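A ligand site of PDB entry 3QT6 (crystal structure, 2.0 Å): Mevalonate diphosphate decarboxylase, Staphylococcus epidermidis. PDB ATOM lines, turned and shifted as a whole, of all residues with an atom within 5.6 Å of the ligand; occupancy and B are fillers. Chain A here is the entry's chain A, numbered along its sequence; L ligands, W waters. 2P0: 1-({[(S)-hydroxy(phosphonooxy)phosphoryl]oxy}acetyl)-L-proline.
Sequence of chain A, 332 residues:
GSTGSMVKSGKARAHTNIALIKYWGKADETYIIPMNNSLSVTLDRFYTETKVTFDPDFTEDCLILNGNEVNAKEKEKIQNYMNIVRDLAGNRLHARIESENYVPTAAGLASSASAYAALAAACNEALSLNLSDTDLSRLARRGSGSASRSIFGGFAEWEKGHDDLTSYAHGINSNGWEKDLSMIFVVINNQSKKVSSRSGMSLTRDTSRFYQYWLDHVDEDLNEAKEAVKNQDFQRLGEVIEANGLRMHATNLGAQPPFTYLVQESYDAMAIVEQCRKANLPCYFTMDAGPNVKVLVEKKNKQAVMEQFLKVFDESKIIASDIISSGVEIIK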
ATOM      1  N   ASN A  17      -4.397  -0.560 -22.981  1.00  0.00           N
ATOM      2  CA  ASN A  17      -5.192   0.136 -21.986  1.00  0.00           C
ATOM      3  C   ASN A  17      -6.367   0.815 -22.668  1.00  0.00           C
ATOM      4  O   ASN A  17      -6.309   1.137 -23.860  1.00  0.00           O
ATOM      5  CB  ASN A  17      -4.356   1.164 -21.224  1.00  0.00           C
ATOM      6  CG  ASN A  17      -3.988   2.364 -22.067  1.00  0.00           C
ATOM      7  OD1 ASN A  17      -4.736   3.332 -22.151  1.00  0.00           O
ATOM      8  ND2 ASN A  17      -2.829   2.315 -22.691  1.00  0.00           N
ATOM      9  N   ALA A  19      -8.894   4.168 -22.305  1.00  0.00           N
ATOM     10  CA  ALA A  19      -9.117   5.457 -21.654  1.00  0.00           C
ATOM     11  C   ALA A  19     -10.551   5.564 -21.134  1.00  0.00           C
ATOM     12  O   ALA A  19     -11.513   5.440 -21.903  1.00  0.00           O
ATOM     13  CB  ALA A  19      -8.816   6.605 -22.620  1.00  0.00           C
ATOM     14  N   LYS A  22     -11.077  10.463 -21.802  1.00  0.00           N
ATOM     15  CA  LYS A  22     -10.502  10.361 -23.147  1.00  0.00           C
ATOM     16  C   LYS A  22      -9.377  11.343 -23.493  1.00  0.00           C
ATOM     17  O   LYS A  22      -9.454  12.546 -23.208  1.00  0.00           O
ATOM     18  CB  LYS A  22     -11.586  10.469 -24.248  1.00  0.00           C
ATOM     19  CG  LYS A  22     -12.750   9.499 -24.126  1.00  0.00           C
ATOM     20  CD  LYS A  22     -12.302   8.057 -24.170  1.00  0.00           C
ATOM     21  CE  LYS A  22     -13.457   7.103 -24.283  1.00  0.00           C
ATOM     22  NZ  LYS A  22     -12.984   5.696 -24.195  1.00  0.00           N
ATOM     23  N   TYR A  23      -8.338  10.789 -24.120  1.00  0.00           N
ATOM     24  CA  TYR A  23      -7.408  11.560 -24.948  1.00  0.00           C
ATOM     25  C   TYR A  23      -8.074  11.773 -26.306  1.00  0.00           C
ATOM     26  O   TYR A  23      -8.431  10.824 -26.978  1.00  0.00           O
ATOM     27  CB  TYR A  23      -6.115  10.739 -25.106  1.00  0.00           C
ATOM     28  CG  TYR A  23      -5.223  11.064 -26.292  1.00  0.00           C
ATOM     29  CD1 TYR A  23      -4.895  12.364 -26.619  1.00  0.00           C
ATOM     30  CD2 TYR A  23      -4.667  10.038 -27.069  1.00  0.00           C
ATOM     31  CE1 TYR A  23      -4.040  12.657 -27.692  1.00  0.00           C
ATOM     32  CE2 TYR A  23      -3.820  10.302 -28.139  1.00  0.00           C
ATOM     33  CZ  TYR A  23      -3.509  11.613 -28.443  1.00  0.00           C
ATOM     34  OH  TYR A  23      -2.689  11.885 -29.502  1.00  0.00           O
ATOM     35  N   TRP A  24      -8.250  13.026 -26.708  1.00  0.00           N
ATOM     36  CA  TRP A  24      -8.865  13.304 -27.999  1.00  0.00           C
ATOM     37  C   TRP A  24      -8.500  14.697 -28.459  1.00  0.00           C
ATOM     38  O   TRP A  24      -9.130  15.679 -28.045  1.00  0.00           O
ATOM     39  CB  TRP A  24     -10.397  13.194 -27.901  1.00  0.00           C
ATOM     40  CG  TRP A  24     -11.046  13.004 -29.240  1.00  0.00           C
ATOM     41  CD1 TRP A  24     -11.943  13.853 -29.852  1.00  0.00           C
ATOM     42  CD2 TRP A  24     -10.845  11.922 -30.143  1.00  0.00           C
ATOM     43  NE1 TRP A  24     -12.310  13.338 -31.074  1.00  0.00           N
ATOM     44  CE2 TRP A  24     -11.643  12.158 -31.278  1.00  0.00           C
ATOM     45  CE3 TRP A  24     -10.062  10.764 -30.102  1.00  0.00           C
ATOM     46  CZ2 TRP A  24     -11.682  11.285 -32.360  1.00  0.00           C
ATOM     47  CZ3 TRP A  24     -10.092   9.893 -31.174  1.00  0.00           C
ATOM     48  CH2 TRP A  24     -10.901  10.161 -32.296  1.00  0.00           C
ATOM     49  N   LYS A  26      -4.727  16.858 -30.122  1.00  0.00           N
ATOM     50  CA  LYS A  26      -3.360  17.185 -29.740  1.00  0.00           C
ATOM     51  C   LYS A  26      -3.081  18.680 -29.777  1.00  0.00           C
ATOM     52  O   LYS A  26      -3.482  19.373 -30.715  1.00  0.00           O
ATOM     53  CB  LYS A  26      -2.354  16.526 -30.688  1.00  0.00           C
ATOM     54  CG  LYS A  26      -2.350  14.995 -30.747  1.00  0.00           C
ATOM     55  CD  LYS A  26      -1.497  14.552 -31.959  1.00  0.00           C
ATOM     56  CE  LYS A  26      -1.387  13.049 -32.115  1.00  0.00           C
ATOM     57  NZ  LYS A  26      -2.707  12.374 -32.279  1.00  0.00           N
ATOM     58  N   GLU A  29       1.307  18.234 -32.804  1.00  0.00           N
ATOM     59  CA  GLU A  29       1.174  17.073 -33.669  1.00  0.00           C
ATOM     60  C   GLU A  29       2.517  16.371 -33.845  1.00  0.00           C
ATOM     61  O   GLU A  29       2.575  15.168 -34.037  1.00  0.00           O
ATOM     62  CB  GLU A  29       0.581  17.474 -35.020  1.00  0.00           C
ATOM     63  CG  GLU A  29       0.306  16.307 -35.950  1.00  0.00           C
ATOM     64  CD  GLU A  29      -0.869  15.437 -35.506  1.00  0.00           C
ATOM     65  OE1 GLU A  29      -1.692  15.917 -34.703  1.00  0.00           O
ATOM     66  OE2 GLU A  29      -0.958  14.285 -35.967  1.00  0.00           O
ATOM     67  N   ILE A  32       3.492  14.800 -30.154  1.00  0.00           N
ATOM     68  CA  ILE A  32       2.341  14.160 -29.546  1.00  0.00           C
ATOM     69  C   ILE A  32       2.076  14.664 -28.116  1.00  0.00           C
ATOM     70  O   ILE A  32       2.190  13.952 -27.126  1.00  0.00           O
ATOM     71  CB  ILE A  32       2.436  12.631 -29.656  1.00  0.00           C
ATOM     72  CG1 ILE A  32       2.625  12.282 -31.142  1.00  0.00           C
ATOM     73  CG2 ILE A  32       1.177  11.961 -29.081  1.00  0.00           C
ATOM     74  CD1 ILE A  32       2.600  10.826 -31.462  1.00  0.00           C
ATOM     75  N   SER A  38      -5.575  12.462 -19.623  1.00  0.00           N
ATOM     76  CA  SER A  38      -6.446  11.308 -19.795  1.00  0.00           C
ATOM     77  C   SER A  38      -6.204  10.303 -18.674  1.00  0.00           C
ATOM     78  O   SER A  38      -5.163  10.315 -18.038  1.00  0.00           O
ATOM     79  CB  SER A  38      -6.264  10.678 -21.178  1.00  0.00           C
ATOM     80  OG  SER A  38      -4.907  10.337 -21.439  1.00  0.00           O
ATOM     81  N   SER A 112      -1.799   0.059 -30.819  1.00  0.00           N
ATOM     82  CA  SER A 112      -0.696   1.013 -30.839  1.00  0.00           C
ATOM     83  C   SER A 112      -0.201   1.306 -29.415  1.00  0.00           C
ATOM     84  O   SER A 112       1.002   1.515 -29.207  1.00  0.00           O
ATOM     85  CB  SER A 112      -1.043   2.295 -31.599  1.00  0.00           C
ATOM     86  OG  SER A 112      -1.961   3.096 -30.874  1.00  0.00           O
ATOM     87  N   GLY A 143       5.648   7.676 -29.994  1.00  0.00           N
ATOM     88  CA  GLY A 143       5.177   6.717 -30.981  1.00  0.00           C
ATOM     89  C   GLY A 143       3.659   6.753 -31.081  1.00  0.00           C
ATOM     90  O   GLY A 143       3.090   6.778 -32.178  1.00  0.00           O
ATOM     91  N   SER A 144       3.009   6.779 -29.932  1.00  0.00           N
ATOM     92  CA  SER A 144       1.567   6.867 -29.900  1.00  0.00           C
ATOM     93  C   SER A 144       1.148   7.390 -28.529  1.00  0.00           C
ATOM     94  O   SER A 144       1.604   6.869 -27.519  1.00  0.00           O
ATOM     95  CB  SER A 144       0.974   5.475 -30.148  1.00  0.00           C
ATOM     96  OG  SER A 144      -0.443   5.504 -30.118  1.00  0.00           O
ATOM     97  N   GLY A 145       0.285   8.403 -28.503  1.00  0.00           N
ATOM     98  CA  GLY A 145      -0.131   9.032 -27.258  1.00  0.00           C
ATOM     99  C   GLY A 145      -0.566   8.050 -26.189  1.00  0.00           C
ATOM    100  O   GLY A 145      -0.063   8.076 -25.072  1.00  0.00           O
ATOM    101  N   SER A 146      -1.507   7.170 -26.529  1.00  0.00           N
ATOM    102  CA  SER A 146      -2.012   6.198 -25.570  1.00  0.00           C
ATOM    103  C   SER A 146      -0.926   5.255 -25.048  1.00  0.00           C
ATOM    104  O   SER A 146      -1.081   4.682 -23.982  1.00  0.00           O
ATOM    105  CB  SER A 146      -3.158   5.398 -26.183  1.00  0.00           C
ATOM    106  OG  SER A 146      -2.803   4.913 -27.476  1.00  0.00           O
ATOM    107  N   ALA A 147       0.146   5.076 -25.808  1.00  0.00           N
ATOM    108  CA  ALA A 147       1.250   4.219 -25.364  1.00  0.00           C
ATOM    109  C   ALA A 147       1.916   4.755 -24.083  1.00  0.00           C
ATOM    110  O   ALA A 147       2.475   3.983 -23.287  1.00  0.00           O
ATOM    111  CB  ALA A 147       2.289   4.046 -26.474  1.00  0.00           C
ATOM    112  N   ARG A 149       0.651   5.573 -21.479  1.00  0.00           N
ATOM    113  CA  ARG A 149      -0.036   5.029 -20.299  1.00  0.00           C
ATOM    114  C   ARG A 149       0.200   3.542 -20.076  1.00  0.00           C
ATOM    115  O   ARG A 149       0.108   3.061 -18.959  1.00  0.00           O
ATOM    116  CB  ARG A 149      -1.543   5.302 -20.386  1.00  0.00           C
ATOM    117  CG  ARG A 149      -1.908   6.792 -20.526  1.00  0.00           C
ATOM    118  CD  ARG A 149      -3.432   7.014 -20.571  1.00  0.00           C
ATOM    119  NE  ARG A 149      -4.063   6.134 -21.547  1.00  0.00           N
ATOM    120  CZ  ARG A 149      -4.644   6.541 -22.673  1.00  0.00           C
ATOM    121  NH1 ARG A 149      -4.718   7.839 -22.955  1.00  0.00           N
ATOM    122  NH2 ARG A 149      -5.164   5.657 -23.508  1.00  0.00           N
ATOM    123  N   TRP A 158      -2.249  10.262 -17.932  1.00  0.00           N
ATOM    124  CA  TRP A 158      -1.341  10.981 -18.788  1.00  0.00           C
ATOM    125  C   TRP A 158      -1.449  12.467 -18.499  1.00  0.00           C
ATOM    126  O   TRP A 158      -2.494  13.081 -18.763  1.00  0.00           O
ATOM    127  CB  TRP A 158      -1.650  10.679 -20.258  1.00  0.00           C
ATOM    128  CG  TRP A 158      -0.773  11.374 -21.243  1.00  0.00           C
ATOM    129  CD1 TRP A 158       0.359  12.082 -20.970  1.00  0.00           C
ATOM    130  CD2 TRP A 158      -0.946  11.403 -22.663  1.00  0.00           C
ATOM    131  NE1 TRP A 158       0.893  12.574 -22.150  1.00  0.00           N
ATOM    132  CE2 TRP A 158       0.100  12.168 -23.203  1.00  0.00           C
ATOM    133  CE3 TRP A 158      -1.900  10.865 -23.544  1.00  0.00           C
ATOM    134  CZ2 TRP A 158       0.234  12.406 -24.558  1.00  0.00           C
ATOM    135  CZ3 TRP A 158      -1.779  11.111 -24.889  1.00  0.00           C
ATOM    136  CH2 TRP A 158      -0.718  11.872 -25.385  1.00  0.00           C
ATOM    137  N   SER A 197      -7.575   7.129 -35.980  1.00  0.00           N
ATOM    138  CA  SER A 197      -7.893   7.962 -34.836  1.00  0.00           C
ATOM    139  C   SER A 197      -7.058   9.248 -34.779  1.00  0.00           C
ATOM    140  O   SER A 197      -7.513  10.264 -34.276  1.00  0.00           O
ATOM    141  CB  SER A 197      -7.725   7.173 -33.530  1.00  0.00           C
ATOM    142  OG  SER A 197      -6.358   6.915 -33.268  1.00  0.00           O
ATOM    143  N   ARG A 198      -5.828   9.197 -35.284  1.00  0.00           N
ATOM    144  CA  ARG A 198      -4.980  10.387 -35.334  1.00  0.00           C
ATOM    145  C   ARG A 198      -5.630  11.403 -36.246  1.00  0.00           C
ATOM    146  O   ARG A 198      -5.723  12.589 -35.926  1.00  0.00           O
ATOM    147  CB  ARG A 198      -3.572  10.032 -35.825  1.00  0.00           C
ATOM    148  CG  ARG A 198      -2.594  11.216 -35.910  1.00  0.00           C
ATOM    149  CD  ARG A 198      -1.159  10.720 -36.145  1.00  0.00           C
ATOM    150  NE  ARG A 198      -0.651   9.913 -35.025  1.00  0.00           N
ATOM    151  CZ  ARG A 198       0.536   9.312 -35.009  1.00  0.00           C
ATOM    152  NH1 ARG A 198       1.345   9.404 -36.053  1.00  0.00           N
ATOM    153  NH2 ARG A 198       0.914   8.594 -33.953  1.00  0.00           N
ATOM    154  N   MET A 201      -9.219  12.606 -34.703  1.00  0.00           N
ATOM    155  CA  MET A 201      -9.082  13.540 -33.604  1.00  0.00           C
ATOM    156  C   MET A 201      -8.534  14.883 -34.080  1.00  0.00           C
ATOM    157  O   MET A 201      -8.878  15.925 -33.527  1.00  0.00           O
ATOM    158  CB  MET A 201      -8.251  12.960 -32.454  1.00  0.00           C
ATOM    159  CG  MET A 201      -6.748  13.017 -32.621  1.00  0.00           C
ATOM    160  SD  MET A 201      -5.924  12.589 -31.059  1.00  0.00           S
ATOM    161  CE  MET A 201      -6.229  10.820 -30.950  1.00  0.00           C
ATOM    162  N   MET A 248     -17.055  12.984 -25.814  1.00  0.00           N
ATOM    163  CA  MET A 248     -15.985  12.869 -26.802  1.00  0.00           C
ATOM    164  C   MET A 248     -16.598  12.565 -28.159  1.00  0.00           C
ATOM    165  O   MET A 248     -16.240  13.180 -29.181  1.00  0.00           O
ATOM    166  CB  MET A 248     -15.008  11.768 -26.411  1.00  0.00           C
ATOM    167  CG  MET A 248     -13.672  11.847 -27.162  1.00  0.00           C
ATOM    168  SD  MET A 248     -13.125  10.225 -27.740  1.00  0.00           S
ATOM    169  CE  MET A 248     -14.305   9.976 -29.062  1.00  0.00           C
ATOM    170  N   MET A 287     -16.604   4.026 -25.522  1.00  0.00           N
ATOM    171  CA  MET A 287     -16.281   3.616 -26.887  1.00  0.00           C
ATOM    172  C   MET A 287     -15.090   4.452 -27.357  1.00  0.00           C
ATOM    173  O   MET A 287     -14.930   5.602 -26.938  1.00  0.00           O
ATOM    174  CB  MET A 287     -17.471   3.863 -27.846  1.00  0.00           C
ATOM    175  CG  MET A 287     -18.685   2.947 -27.652  1.00  0.00           C
ATOM    176  SD  MET A 287     -19.708   3.389 -26.227  1.00  0.00           S
ATOM    177  CE  MET A 287     -20.067   5.122 -26.548  1.00  0.00           C
ATOM    178  N   ASP A 288     -14.267   3.874 -28.219  1.00  0.00           N
ATOM    179  CA  ASP A 288     -13.096   4.572 -28.732  1.00  0.00           C
ATOM    180  C   ASP A 288     -13.254   4.941 -30.217  1.00  0.00           C
ATOM    181  O   ASP A 288     -14.352   5.319 -30.647  1.00  0.00           O
ATOM    182  CB  ASP A 288     -11.827   3.767 -28.420  1.00  0.00           C
ATOM    183  CG  ASP A 288     -11.517   3.729 -26.918  1.00  0.00           C
ATOM    184  OD1 ASP A 288     -11.397   4.820 -26.312  1.00  0.00           O
ATOM    185  OD2 ASP A 288     -11.424   2.639 -26.332  1.00  0.00           O
ATOM    186  N   ALA A 289     -12.183   4.857 -31.003  1.00  0.00           N
ATOM    187  CA  ALA A 289     -12.235   5.220 -32.418  1.00  0.00           C
ATOM    188  C   ALA A 289     -12.892   4.138 -33.250  1.00  0.00           C
ATOM    189  O   ALA A 289     -12.392   3.792 -34.326  1.00  0.00           O
ATOM    190  CB  ALA A 289     -10.831   5.522 -32.948  1.00  0.00           C
HETATM  191  C   2P0 L   1      -7.231   6.780 -26.337  1.00  0.00           C
HETATM  192  N   2P0 L   1      -8.341   7.094 -28.432  1.00  0.00           N
HETATM  193  O   2P0 L   1      -6.489   7.244 -25.420  1.00  0.00           O
HETATM  194  CA  2P0 L   1      -8.022   7.698 -27.176  1.00  0.00           C
HETATM  195  CB  2P0 L   1      -9.307   7.997 -26.507  1.00  0.00           C
HETATM  196  CD  2P0 L   1      -9.706   6.695 -28.465  1.00  0.00           C
HETATM  197  CG  2P0 L   1     -10.393   7.557 -27.461  1.00  0.00           C
HETATM  198  OAB 2P0 L   1      -7.888   6.350 -30.528  1.00  0.00           O
HETATM  199  OAC 2P0 L   1      -2.207   9.914 -32.750  1.00  0.00           O
HETATM  200  OAD 2P0 L   1      -3.203   5.698 -31.409  1.00  0.00           O
HETATM  201  OAF 2P0 L   1      -1.484   9.612 -30.408  1.00  0.00           O
HETATM  202  OAG 2P0 L   1      -1.040   7.848 -31.982  1.00  0.00           O
HETATM  203  OAH 2P0 L   1      -3.132   6.887 -29.205  1.00  0.00           O
HETATM  204  CAK 2P0 L   1      -6.020   7.296 -29.482  1.00  0.00           C
HETATM  205  OAM 2P0 L   1      -5.259   6.725 -30.497  1.00  0.00           O
HETATM  206  OAN 2P0 L   1      -3.438   8.250 -31.324  1.00  0.00           O
HETATM  207  CAP 2P0 L   1      -7.452   6.883 -29.529  1.00  0.00           C
HETATM  208  PAS 2P0 L   1      -2.044   8.927 -31.630  1.00  0.00           P
HETATM  209  PAT 2P0 L   1      -3.708   6.866 -30.617  1.00  0.00           P
HETATM  210  OXT 2P0 L   1      -7.263   5.524 -26.498  1.00  0.00           O
HETATM  211  O   HOH W   1      -5.733   3.268 -25.831  1.00  0.00           O
HETATM  212  O   HOH W   2      -8.916   4.078 -25.266  1.00  0.00           O
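Merely in contact with the ligand: Asp 288 (3.1 Å), Ala 19 (3.7 Å), Ile 32 (3.8 Å), Lys 22 (3.8 Å), Met 201 (3.8 Å), Met 248 (3.8 Å) and Ala 289 (3.9 Å).
Within 4 Å of the ligand: Ala 19, Lys 22, Tyr 23, Lys 26, Ile 32, Ser 112, Ser 144, Gly 145, Ser 146, Arg 149, Ser 197, Arg 198, Met 201, Met 248, Asp 288 and Ala 289.
The nearest printed residue that does not touch the ligand is Trp 24 (4.2 Å).
The backbone carbonyl oxygen (O) of Ser 146 is in hydrogen-bond range of the side-chain amide nitrogen (ND2) of Asn 17 (3.2 Å).
SD of Met 201 sits at hydrogen-bond distance from OH of Tyr 23 (3.7 Å).
The backbone carbonyl oxygen (O) of Gly 143 sits at hydrogen-bond distance from the guanidinium group (NH2) of Arg 198, 3.3 Å away.
The guanidinium group (NH2) of Arg 149 lies within hydrogen-bond range of the side-chain amide oxygen (OD1) of Asn 17.
OG of Ser 112 lies within hydrogen-bond range of OG of Ser 144, at 2.9 Å.
OD1 of Asp 288 is in salt-bridge range of NZ of Lys 22 (2.8 Å).
The backbone carbonyl oxygen of Ala 19 is in hydrogen-bond range of the side-chain amino group of Lys 22 (2.7 Å).
O of Met 287 is in hydrogen-bond range of NZ of Lys 22 (3.4 Å).
Water W2 lies within hydrogen-bond range of an oxygen (OXT) of the ligand (2.5 Å), the side-chain carboxylate (OD1) of Asp 288 (2.8 Å) and the backbone NH (N) of Ala 19 (3.0 Å).
Water W1 lies within hydrogen-bond range of an oxygen (OXT) of the ligand, the backbone carbonyl oxygen of Asn 17 and the guanidinium group of Arg 149.
The side-chain amino group (NZ) of Lys 26 lies within salt-bridge range of an oxygen (OAC) of the ligand (2.6 Å).
The backbone NH (N) of Ser 146 lies within hydrogen-bond range of an oxygen (OAH) of the ligand, 3.1 Å away.
OAH of the ligand is in hydrogen-bond range of OG of Ser 146, 2.6 Å away.
OAF of the ligand lies within hydrogen-bond range of OH of Tyr 23 (2.7 Å).
The guanidinium group (NE) of Arg 198 lies within salt-bridge range of an oxygen (OAC) of the ligand, at 2.8 Å.
O of the ligand lies within salt-bridge range of NH2 of Arg 149 (2.8 Å).
An oxygen (OAF) of the ligand sits at hydrogen-bond distance from the backbone NH (N) of Gly 145 (2.9 Å).
The side-chain hydroxyl (OG) of Ser 112 lies within hydrogen-bond range of an oxygen (OAD) of the ligand, at 2.9 Å.
The side-chain hydroxyl (OG) of Ser 197 sits at hydrogen-bond distance from an oxygen (OAM) of the ligand (3.0 Å).
An oxygen (OAD) of the ligand is in hydrogen-bond range of the side-chain hydroxyl (OG) of Ser 144 (3.1 Å).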
